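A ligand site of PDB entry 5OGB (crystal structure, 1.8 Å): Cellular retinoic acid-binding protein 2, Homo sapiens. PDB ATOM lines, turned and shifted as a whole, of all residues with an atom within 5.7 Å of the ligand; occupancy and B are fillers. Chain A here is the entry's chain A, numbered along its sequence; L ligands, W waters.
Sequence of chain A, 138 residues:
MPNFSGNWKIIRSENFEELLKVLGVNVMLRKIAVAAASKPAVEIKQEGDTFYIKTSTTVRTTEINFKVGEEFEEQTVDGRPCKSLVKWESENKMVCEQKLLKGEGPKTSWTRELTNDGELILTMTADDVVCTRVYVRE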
ATOM      1  N   ILE A  10       2.456   8.485  25.238  1.00  0.00           N
ATOM      2  CA  ILE A  10       1.988   8.826  26.574  1.00  0.00           C
ATOM      3  C   ILE A  10       1.402   7.625  27.351  1.00  0.00           C
ATOM      4  O   ILE A  10       0.637   6.835  26.769  1.00  0.00           O
ATOM      5  CB  ILE A  10       1.032  10.069  26.557  1.00  0.00           C
ATOM      6  CG1 ILE A  10       0.960  10.651  27.957  1.00  0.00           C
ATOM      7  CG2 ILE A  10      -0.351   9.734  26.068  1.00  0.00           C
ATOM      8  CD1 ILE A  10       0.421  12.021  28.019  1.00  0.00           C
ATOM      9  N   PHE A  16      -3.318  18.027  33.693  1.00  0.00           N
ATOM     10  CA  PHE A  16      -3.301  18.794  32.427  1.00  0.00           C
ATOM     11  C   PHE A  16      -4.508  19.718  32.305  1.00  0.00           C
ATOM     12  O   PHE A  16      -4.360  20.907  32.021  1.00  0.00           O
ATOM     13  CB  PHE A  16      -3.223  17.903  31.169  1.00  0.00           C
ATOM     14  CG  PHE A  16      -3.058  18.700  29.891  1.00  0.00           C
ATOM     15  CD1 PHE A  16      -1.999  19.561  29.730  1.00  0.00           C
ATOM     16  CD2 PHE A  16      -3.993  18.597  28.865  1.00  0.00           C
ATOM     17  CE1 PHE A  16      -1.853  20.306  28.560  1.00  0.00           C
ATOM     18  CE2 PHE A  16      -3.853  19.335  27.691  1.00  0.00           C
ATOM     19  CZ  PHE A  16      -2.794  20.191  27.539  1.00  0.00           C
ATOM     20  N   LEU A  20      -4.684  23.953  32.398  1.00  0.00           N
ATOM     21  CA  LEU A  20      -5.395  24.795  31.470  1.00  0.00           C
ATOM     22  C   LEU A  20      -6.491  25.602  32.191  1.00  0.00           C
ATOM     23  O   LEU A  20      -6.728  26.769  31.847  1.00  0.00           O
ATOM     24  CB  LEU A  20      -6.000  23.961  30.318  1.00  0.00           C
ATOM     25  CG  LEU A  20      -5.062  23.216  29.338  1.00  0.00           C
ATOM     26  CD1 LEU A  20      -5.848  22.506  28.290  1.00  0.00           C
ATOM     27  CD2 LEU A  20      -4.044  24.123  28.678  1.00  0.00           C
ATOM     28  N   VAL A  25      -8.349  28.958  30.266  1.00  0.00           N
ATOM     29  CA  VAL A  25      -8.708  28.541  28.952  1.00  0.00           C
ATOM     30  C   VAL A  25     -10.186  28.248  28.975  1.00  0.00           C
ATOM     31  O   VAL A  25     -10.721  27.621  29.889  1.00  0.00           O
ATOM     32  CB  VAL A  25      -7.859  27.332  28.507  1.00  0.00           C
ATOM     33  CG1 VAL A  25      -8.363  26.778  27.189  1.00  0.00           C
ATOM     34  CG2 VAL A  25      -6.389  27.739  28.471  1.00  0.00           C
ATOM     35  N   LEU A  29     -12.838  25.155  24.460  1.00  0.00           N
ATOM     36  CA  LEU A  29     -11.524  24.878  23.914  1.00  0.00           C
ATOM     37  C   LEU A  29     -10.774  23.893  24.815  1.00  0.00           C
ATOM     38  O   LEU A  29     -10.049  23.067  24.328  1.00  0.00           O
ATOM     39  CB  LEU A  29     -10.728  26.171  23.748  1.00  0.00           C
ATOM     40  CG  LEU A  29     -11.309  27.171  22.744  1.00  0.00           C
ATOM     41  CD1 LEU A  29     -10.337  28.315  22.541  1.00  0.00           C
ATOM     42  CD2 LEU A  29     -11.580  26.460  21.420  1.00  0.00           C
ATOM     43  N   ARG A  30     -10.979  23.981  26.123  1.00  0.00           N
ATOM     44  CA  ARG A  30     -10.275  23.117  27.072  1.00  0.00           C
ATOM     45  C   ARG A  30     -10.593  21.655  26.824  1.00  0.00           C
ATOM     46  O   ARG A  30      -9.711  20.860  26.793  1.00  0.00           O
ATOM     47  CB  ARG A  30     -10.632  23.505  28.510  1.00  0.00           C
ATOM     48  CG  ARG A  30      -9.587  23.113  29.521  1.00  0.00           C
ATOM     49  CD  ARG A  30      -9.909  23.664  30.882  1.00  0.00           C
ATOM     50  NE  ARG A  30     -11.144  23.130  31.456  1.00  0.00           N
ATOM     51  CZ  ARG A  30     -12.145  23.834  31.990  1.00  0.00           C
ATOM     52  NH1 ARG A  30     -12.167  25.175  31.979  1.00  0.00           N
ATOM     53  NH2 ARG A  30     -13.172  23.174  32.541  1.00  0.00           N
ATOM     54  N   ILE A  32     -11.489  20.189  23.998  1.00  0.00           N
ATOM     55  CA  ILE A  32     -10.810  19.812  22.741  1.00  0.00           C
ATOM     56  C   ILE A  32      -9.318  19.644  23.048  1.00  0.00           C
ATOM     57  O   ILE A  32      -8.751  18.657  22.704  1.00  0.00           O
ATOM     58  CB  ILE A  32     -11.027  20.814  21.586  1.00  0.00           C
ATOM     59  CG1 ILE A  32     -12.511  20.911  21.178  1.00  0.00           C
ATOM     60  CG2 ILE A  32     -10.227  20.380  20.356  1.00  0.00           C
ATOM     61  CD1 ILE A  32     -12.848  22.204  20.486  1.00  0.00           C
ATOM     62  N   ALA A  33      -8.698  20.573  23.779  1.00  0.00           N
ATOM     63  CA  ALA A  33      -7.263  20.475  24.114  1.00  0.00           C
ATOM     64  C   ALA A  33      -6.911  19.218  24.933  1.00  0.00           C
ATOM     65  O   ALA A  33      -5.877  18.559  24.673  1.00  0.00           O
ATOM     66  CB  ALA A  33      -6.822  21.727  24.859  1.00  0.00           C
ATOM     67  N   ALA A  36      -7.235  16.025  22.684  1.00  0.00           N
ATOM     68  CA  ALA A  36      -6.116  15.991  21.729  1.00  0.00           C
ATOM     69  C   ALA A  36      -4.805  15.609  22.427  1.00  0.00           C
ATOM     70  O   ALA A  36      -4.033  14.766  21.931  1.00  0.00           O
ATOM     71  CB  ALA A  36      -5.985  17.336  21.037  1.00  0.00           C
ATOM     72  N   ALA A  37      -4.610  16.163  23.619  1.00  0.00           N
ATOM     73  CA  ALA A  37      -3.458  15.864  24.456  1.00  0.00           C
ATOM     74  C   ALA A  37      -3.460  14.469  25.040  1.00  0.00           C
ATOM     75  O   ALA A  37      -2.427  14.048  25.519  1.00  0.00           O
ATOM     76  CB  ALA A  37      -3.330  16.894  25.571  1.00  0.00           C
ATOM     77  N   PRO A  40      -0.991  12.351  21.948  1.00  0.00           N
ATOM     78  CA  PRO A  40      -0.069  13.047  21.088  1.00  0.00           C
ATOM     79  C   PRO A  40       0.978  12.112  20.452  1.00  0.00           C
ATOM     80  O   PRO A  40       1.219  10.993  20.942  1.00  0.00           O
ATOM     81  CB  PRO A  40       0.641  13.992  22.065  1.00  0.00           C
ATOM     82  CG  PRO A  40       0.702  13.236  23.328  1.00  0.00           C
ATOM     83  CD  PRO A  40      -0.487  12.303  23.337  1.00  0.00           C
ATOM     84  N   VAL A  42       4.864  12.163  19.716  1.00  0.00           N
ATOM     85  CA  VAL A  42       6.054  12.896  20.183  1.00  0.00           C
ATOM     86  C   VAL A  42       7.277  12.290  19.482  1.00  0.00           C
ATOM     87  O   VAL A  42       7.418  11.049  19.451  1.00  0.00           O
ATOM     88  CB  VAL A  42       6.179  12.872  21.703  1.00  0.00           C
ATOM     89  CG1 VAL A  42       7.436  13.597  22.166  1.00  0.00           C
ATOM     90  CG2 VAL A  42       4.981  13.543  22.361  1.00  0.00           C
ATOM     91  N   THR A  55       5.879  17.765  19.129  1.00  0.00           N
ATOM     92  CA  THR A  55       4.689  17.187  19.736  1.00  0.00           C
ATOM     93  C   THR A  55       3.496  17.500  18.860  1.00  0.00           C
ATOM     94  O   THR A  55       3.175  18.678  18.719  1.00  0.00           O
ATOM     95  CB  THR A  55       4.439  17.751  21.143  1.00  0.00           C
ATOM     96  OG1 THR A  55       5.549  17.400  21.982  1.00  0.00           O
ATOM     97  CG2 THR A  55       3.145  17.169  21.733  1.00  0.00           C
ATOM     98  N   THR A  57      -0.582  16.974  17.611  1.00  0.00           N
ATOM     99  CA  THR A  57      -2.002  16.609  17.721  1.00  0.00           C
ATOM    100  C   THR A  57      -2.672  17.393  16.584  1.00  0.00           C
ATOM    101  O   THR A  57      -2.134  18.390  16.103  1.00  0.00           O
ATOM    102  CB  THR A  57      -2.654  17.021  19.069  1.00  0.00           C
ATOM    103  OG1 THR A  57      -2.806  18.450  19.132  1.00  0.00           O
ATOM    104  CG2 THR A  57      -1.810  16.612  20.274  1.00  0.00           C
ATOM    105  N   VAL A  59      -5.009  19.508  16.454  1.00  0.00           N
ATOM    106  CA  VAL A  59      -5.408  20.844  16.779  1.00  0.00           C
ATOM    107  C   VAL A  59      -4.245  21.666  17.299  1.00  0.00           C
ATOM    108  O   VAL A  59      -4.381  22.865  17.457  1.00  0.00           O
ATOM    109  CB  VAL A  59      -6.652  20.880  17.755  1.00  0.00           C
ATOM    110  CG1 VAL A  59      -7.882  20.225  17.100  1.00  0.00           C
ATOM    111  CG2 VAL A  59      -6.386  20.207  19.122  1.00  0.00           C
ATOM    112  N   ARG A  60      -3.070  21.042  17.509  1.00  0.00           N
ATOM    113  CA  ARG A  60      -1.882  21.813  17.940  1.00  0.00           C
ATOM    114  C   ARG A  60      -0.629  20.989  17.798  1.00  0.00           C
ATOM    115  O   ARG A  60      -0.502  19.892  18.379  1.00  0.00           O
ATOM    116  CB  ARG A  60      -1.993  22.278  19.396  1.00  0.00           C
ATOM    117  CG  ARG A  60      -1.132  23.494  19.677  1.00  0.00           C
ATOM    118  CD  ARG A  60      -0.757  23.550  21.112  1.00  0.00           C
ATOM    119  NE  ARG A  60       0.068  24.709  21.462  1.00  0.00           N
ATOM    120  CZ  ARG A  60       0.313  25.112  22.717  1.00  0.00           C
ATOM    121  NH1 ARG A  60      -0.208  24.439  23.755  1.00  0.00           N
ATOM    122  NH2 ARG A  60       1.056  26.202  22.941  1.00  0.00           N
ATOM    123  N   GLN A  75       5.388  28.993  22.351  1.00  0.00           N
ATOM    124  CA  GLN A  75       4.188  29.466  23.031  1.00  0.00           C
ATOM    125  C   GLN A  75       4.138  28.801  24.381  1.00  0.00           C
ATOM    126  O   GLN A  75       4.602  27.668  24.541  1.00  0.00           O
ATOM    127  CB  GLN A  75       2.936  29.071  22.240  1.00  0.00           C
ATOM    128  CG  GLN A  75       2.632  30.000  21.062  1.00  0.00           C
ATOM    129  CD  GLN A  75       1.283  29.709  20.413  1.00  0.00           C
ATOM    130  OE1 GLN A  75       0.574  28.785  20.792  1.00  0.00           O
ATOM    131  NE2 GLN A  75       0.914  30.513  19.449  1.00  0.00           N
ATOM    132  N   THR A  76       3.562  29.479  25.367  1.00  0.00           N
ATOM    133  CA  THR A  76       3.157  28.796  26.590  1.00  0.00           C
ATOM    134  C   THR A  76       2.093  27.681  26.317  1.00  0.00           C
ATOM    135  O   THR A  76       1.544  27.555  25.219  1.00  0.00           O
ATOM    136  CB  THR A  76       2.596  29.798  27.655  1.00  0.00           C
ATOM    137  OG1 THR A  76       1.467  30.482  27.109  1.00  0.00           O
ATOM    138  CG2 THR A  76       3.652  30.807  28.061  1.00  0.00           C
ATOM    139  N   VAL A  77       1.843  26.860  27.309  1.00  0.00           N
ATOM    140  CA  VAL A  77       0.866  25.775  27.174  1.00  0.00           C
ATOM    141  C   VAL A  77      -0.540  26.290  26.752  1.00  0.00           C
ATOM    142  O   VAL A  77      -1.250  25.599  26.010  1.00  0.00           O
ATOM    143  CB  VAL A  77       0.830  24.920  28.468  1.00  0.00           C
ATOM    144  CG1 VAL A  77       0.335  25.730  29.641  1.00  0.00           C
ATOM    145  CG2 VAL A  77       0.008  23.653  28.286  1.00  0.00           C
ATOM    146  N   ASP A  78      -0.895  27.498  27.223  1.00  0.00           N
ATOM    147  CA  ASP A  78      -2.184  28.135  26.936  1.00  0.00           C
ATOM    148  C   ASP A  78      -2.136  29.049  25.714  1.00  0.00           C
ATOM    149  O   ASP A  78      -3.105  29.768  25.474  1.00  0.00           O
ATOM    150  CB  ASP A  78      -2.748  28.891  28.145  1.00  0.00           C
ATOM    151  CG  ASP A  78      -1.861  30.033  28.604  1.00  0.00           C
ATOM    152  OD1 ASP A  78      -0.636  29.791  28.823  1.00  0.00           O
ATOM    153  OD2 ASP A  78      -2.383  31.151  28.771  1.00  0.00           O
ATOM    154  N   GLY A  79      -1.029  29.056  24.981  1.00  0.00           N
ATOM    155  CA  GLY A  79      -1.000  29.665  23.632  1.00  0.00           C
ATOM    156  C   GLY A  79      -0.455  31.077  23.484  1.00  0.00           C
ATOM    157  O   GLY A  79      -0.656  31.686  22.431  1.00  0.00           O
ATOM    158  N   ARG A 112      12.006  18.274  31.468  1.00  0.00           N
ATOM    159  CA  ARG A 112      11.984  16.924  30.957  1.00  0.00           C
ATOM    160  C   ARG A 112      13.148  16.145  31.563  1.00  0.00           C
ATOM    161  O   ARG A 112      14.240  16.654  31.740  1.00  0.00           O
ATOM    162  CB  ARG A 112      12.010  16.877  29.400  1.00  0.00           C
ATOM    163  CG  ARG A 112      10.777  17.365  28.709  1.00  0.00           C
ATOM    164  CD  ARG A 112      10.967  17.349  27.188  1.00  0.00           C
ATOM    165  NE  ARG A 112       9.665  17.293  26.471  1.00  0.00           N
ATOM    166  CZ  ARG A 112       9.013  18.346  25.999  1.00  0.00           C
ATOM    167  NH1 ARG A 112       9.509  19.597  26.103  1.00  0.00           N
ATOM    168  NH2 ARG A 112       7.853  18.134  25.369  1.00  0.00           N
ATOM    169  N   LEU A 122       7.704  14.596  31.746  1.00  0.00           N
ATOM    170  CA  LEU A 122       7.500  16.003  31.431  1.00  0.00           C
ATOM    171  C   LEU A 122       6.743  16.663  32.564  1.00  0.00           C
ATOM    172  O   LEU A 122       5.704  16.169  32.959  1.00  0.00           O
ATOM    173  CB  LEU A 122       6.717  16.136  30.109  1.00  0.00           C
ATOM    174  CG  LEU A 122       6.204  17.538  29.676  1.00  0.00           C
ATOM    175  CD1 LEU A 122       7.305  18.522  29.311  1.00  0.00           C
ATOM    176  CD2 LEU A 122       5.188  17.454  28.520  1.00  0.00           C
ATOM    177  N   MET A 124       4.957  20.468  33.412  1.00  0.00           N
ATOM    178  CA  MET A 124       4.627  21.853  32.975  1.00  0.00           C
ATOM    179  C   MET A 124       3.977  22.584  34.154  1.00  0.00           C
ATOM    180  O   MET A 124       3.058  22.041  34.744  1.00  0.00           O
ATOM    181  CB  MET A 124       3.703  21.861  31.783  1.00  0.00           C
ATOM    182  CG  MET A 124       4.238  21.138  30.535  1.00  0.00           C
ATOM    183  SD  MET A 124       3.064  21.136  29.154  1.00  0.00           S
ATOM    184  CE  MET A 124       2.107  19.699  29.462  1.00  0.00           C
ATOM    185  N   ARG A 133       3.375  14.440  33.059  1.00  0.00           N
ATOM    186  CA  ARG A 133       3.078  13.503  31.995  1.00  0.00           C
ATOM    187  C   ARG A 133       4.281  12.552  31.822  1.00  0.00           C
ATOM    188  O   ARG A 133       5.434  12.973  31.831  1.00  0.00           O
ATOM    189  CB  ARG A 133       2.766  14.306  30.729  1.00  0.00           C
ATOM    190  CG  ARG A 133       1.405  15.028  30.877  1.00  0.00           C
ATOM    191  CD  ARG A 133       1.182  16.115  29.843  1.00  0.00           C
ATOM    192  NE  ARG A 133       1.062  15.638  28.477  1.00  0.00           N
ATOM    193  CZ  ARG A 133      -0.074  15.213  27.906  1.00  0.00           C
ATOM    194  NH1 ARG A 133      -1.213  15.163  28.587  1.00  0.00           N
ATOM    195  NH2 ARG A 133      -0.069  14.832  26.637  1.00  0.00           N
ATOM    196  N   TYR A 135       5.921   9.279  29.608  1.00  0.00           N
ATOM    197  CA  TYR A 135       5.955   8.656  28.276  1.00  0.00           C
ATOM    198  C   TYR A 135       6.957   7.559  28.277  1.00  0.00           C
ATOM    199  O   TYR A 135       7.928   7.585  29.036  1.00  0.00           O
ATOM    200  CB  TYR A 135       6.391   9.627  27.170  1.00  0.00           C
ATOM    201  CG  TYR A 135       5.647  10.945  27.147  1.00  0.00           C
ATOM    202  CD1 TYR A 135       5.866  11.905  28.117  1.00  0.00           C
ATOM    203  CD2 TYR A 135       4.760  11.236  26.139  1.00  0.00           C
ATOM    204  CE1 TYR A 135       5.192  13.092  28.099  1.00  0.00           C
ATOM    205  CE2 TYR A 135       4.075  12.451  26.113  1.00  0.00           C
ATOM    206  CZ  TYR A 135       4.318  13.375  27.110  1.00  0.00           C
ATOM    207  OH  TYR A 135       3.662  14.587  27.142  1.00  0.00           O
HETATM  208  C1  LIG L   1      -4.244  21.830  22.350  1.00  0.00           C
HETATM  209  C2  LIG L   1      -7.263  24.949  19.289  1.00  0.00           C
HETATM  210  C3  LIG L   1      -3.454  22.329  23.387  1.00  0.00           C
HETATM  211  C4  LIG L   1      -3.654  23.631  23.827  1.00  0.00           C
HETATM  212  C5  LIG L   1      -3.599  26.669  23.569  1.00  0.00           C
HETATM  213  C6  LIG L   1      -4.885  25.846  23.780  1.00  0.00           C
HETATM  214  C7  LIG L   1      -6.056  26.499  23.086  1.00  0.00           C
HETATM  215  C8  LIG L   1      -6.732  25.915  22.106  1.00  0.00           C
HETATM  216  C9  LIG L   1      -5.210  25.806  25.288  1.00  0.00           C
HETATM  217  C10 LIG L   1      -7.310  24.107  20.532  1.00  0.00           C
HETATM  218  C11 LIG L   1      -8.710  23.778  20.967  1.00  0.00           C
HETATM  219  N1  LIG L   1      -6.470  24.679  21.662  1.00  0.00           N
HETATM  220  C12 LIG L   1      -5.226  22.592  21.809  1.00  0.00           C
HETATM  221  C13 LIG L   1      -4.654  24.431  23.273  1.00  0.00           C
HETATM  222  C14 LIG L   1      -5.425  23.905  22.232  1.00  0.00           C
HETATM  223  C15 LIG L   1      -2.392  21.488  23.836  1.00  0.00           C
HETATM  224  C16 LIG L   1      -1.516  20.782  24.174  1.00  0.00           C
HETATM  225  C17 LIG L   1      -0.465  19.881  24.551  1.00  0.00           C
HETATM  226  C18 LIG L   1      -0.557  18.567  24.095  1.00  0.00           C
HETATM  227  C19 LIG L   1       0.437  17.644  24.376  1.00  0.00           C
HETATM  228  C20 LIG L   1       1.567  18.040  25.093  1.00  0.00           C
HETATM  229  C21 LIG L   1       1.673  19.356  25.551  1.00  0.00           C
HETATM  230  C22 LIG L   1       0.665  20.277  25.269  1.00  0.00           C
HETATM  231  C23 LIG L   1       2.609  17.041  25.365  1.00  0.00           C
HETATM  232  O1  LIG L   1       3.765  17.453  25.544  1.00  0.00           O
HETATM  233  O2  LIG L   1       2.260  15.820  25.319  1.00  0.00           O
HETATM  234  O   HOH W   1       4.656  19.653  24.607  1.00  0.00           O
HETATM  235  O   HOH W   2       5.902  16.293  24.432  1.00  0.00           O
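The side-chain hydroxyl of Tyr 135 sits at hydrogen-bond distance from an oxygen (O2) of the ligand, 2.6 Å away.
The guanidinium group (NH2) of Arg 133 is in salt-bridge range of an oxygen (O2) of the ligand (2.9 Å).
NE of Arg 133 sits at hydrogen-bond distance from OH of Tyr 135 (3.1 Å).
The backbone carbonyl oxygen of Arg 133 sits at hydrogen-bond distance from the backbone NH of Leu 122, at 2.8 Å.
The guanidinium group (NH2) of Arg 133 sits at hydrogen-bond distance from the backbone carbonyl oxygen (O) of Ala 37 (2.7 Å).
OD1 of Asp 78 is in hydrogen-bond range of OG1 of Thr 76, 2.8 Å away.
O of Arg 60 sits at hydrogen-bond distance from OG1 of Thr 57 (2.8 Å).
The guanidinium group of Arg 60 lies within hydrogen-bond range of the side-chain amide oxygen of Gln 75 (3.4 Å).
The guanidinium group (NH2) of Arg 60 lies within hydrogen-bond range of the backbone carbonyl oxygen (O) of Thr 76, at 2.7 Å.
N of Val 25 sits at hydrogen-bond distance from O of Leu 20 (3.1 Å).
Residues that only touch the ligand: Phe 16, Leu 20, Val 25, Leu 29, Ile 32, Ala 33, Ala 37, Pro 40, Thr 55, Val 59, Arg 60, Val 77, Asp 78, Gly 79, Leu 122 and Met 124.
Hydrophobic or aromatic side chains within 4 Å of the ligand: Phe 16, Leu 20, Val 25, Leu 29, Ile 32, Ala 33, Ala 37, Pro 40, Val 59, Leu 122, Met 124 and Tyr 135.
The nearest printed residue that does not touch the ligand is Arg 112 (4.1 Å).
Water W2 lies within hydrogen-bond range of O1 of the ligand (2.7 Å), OG1 of Thr 55 (2.7 Å) and NH2 of Arg 112 (2.8 Å).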
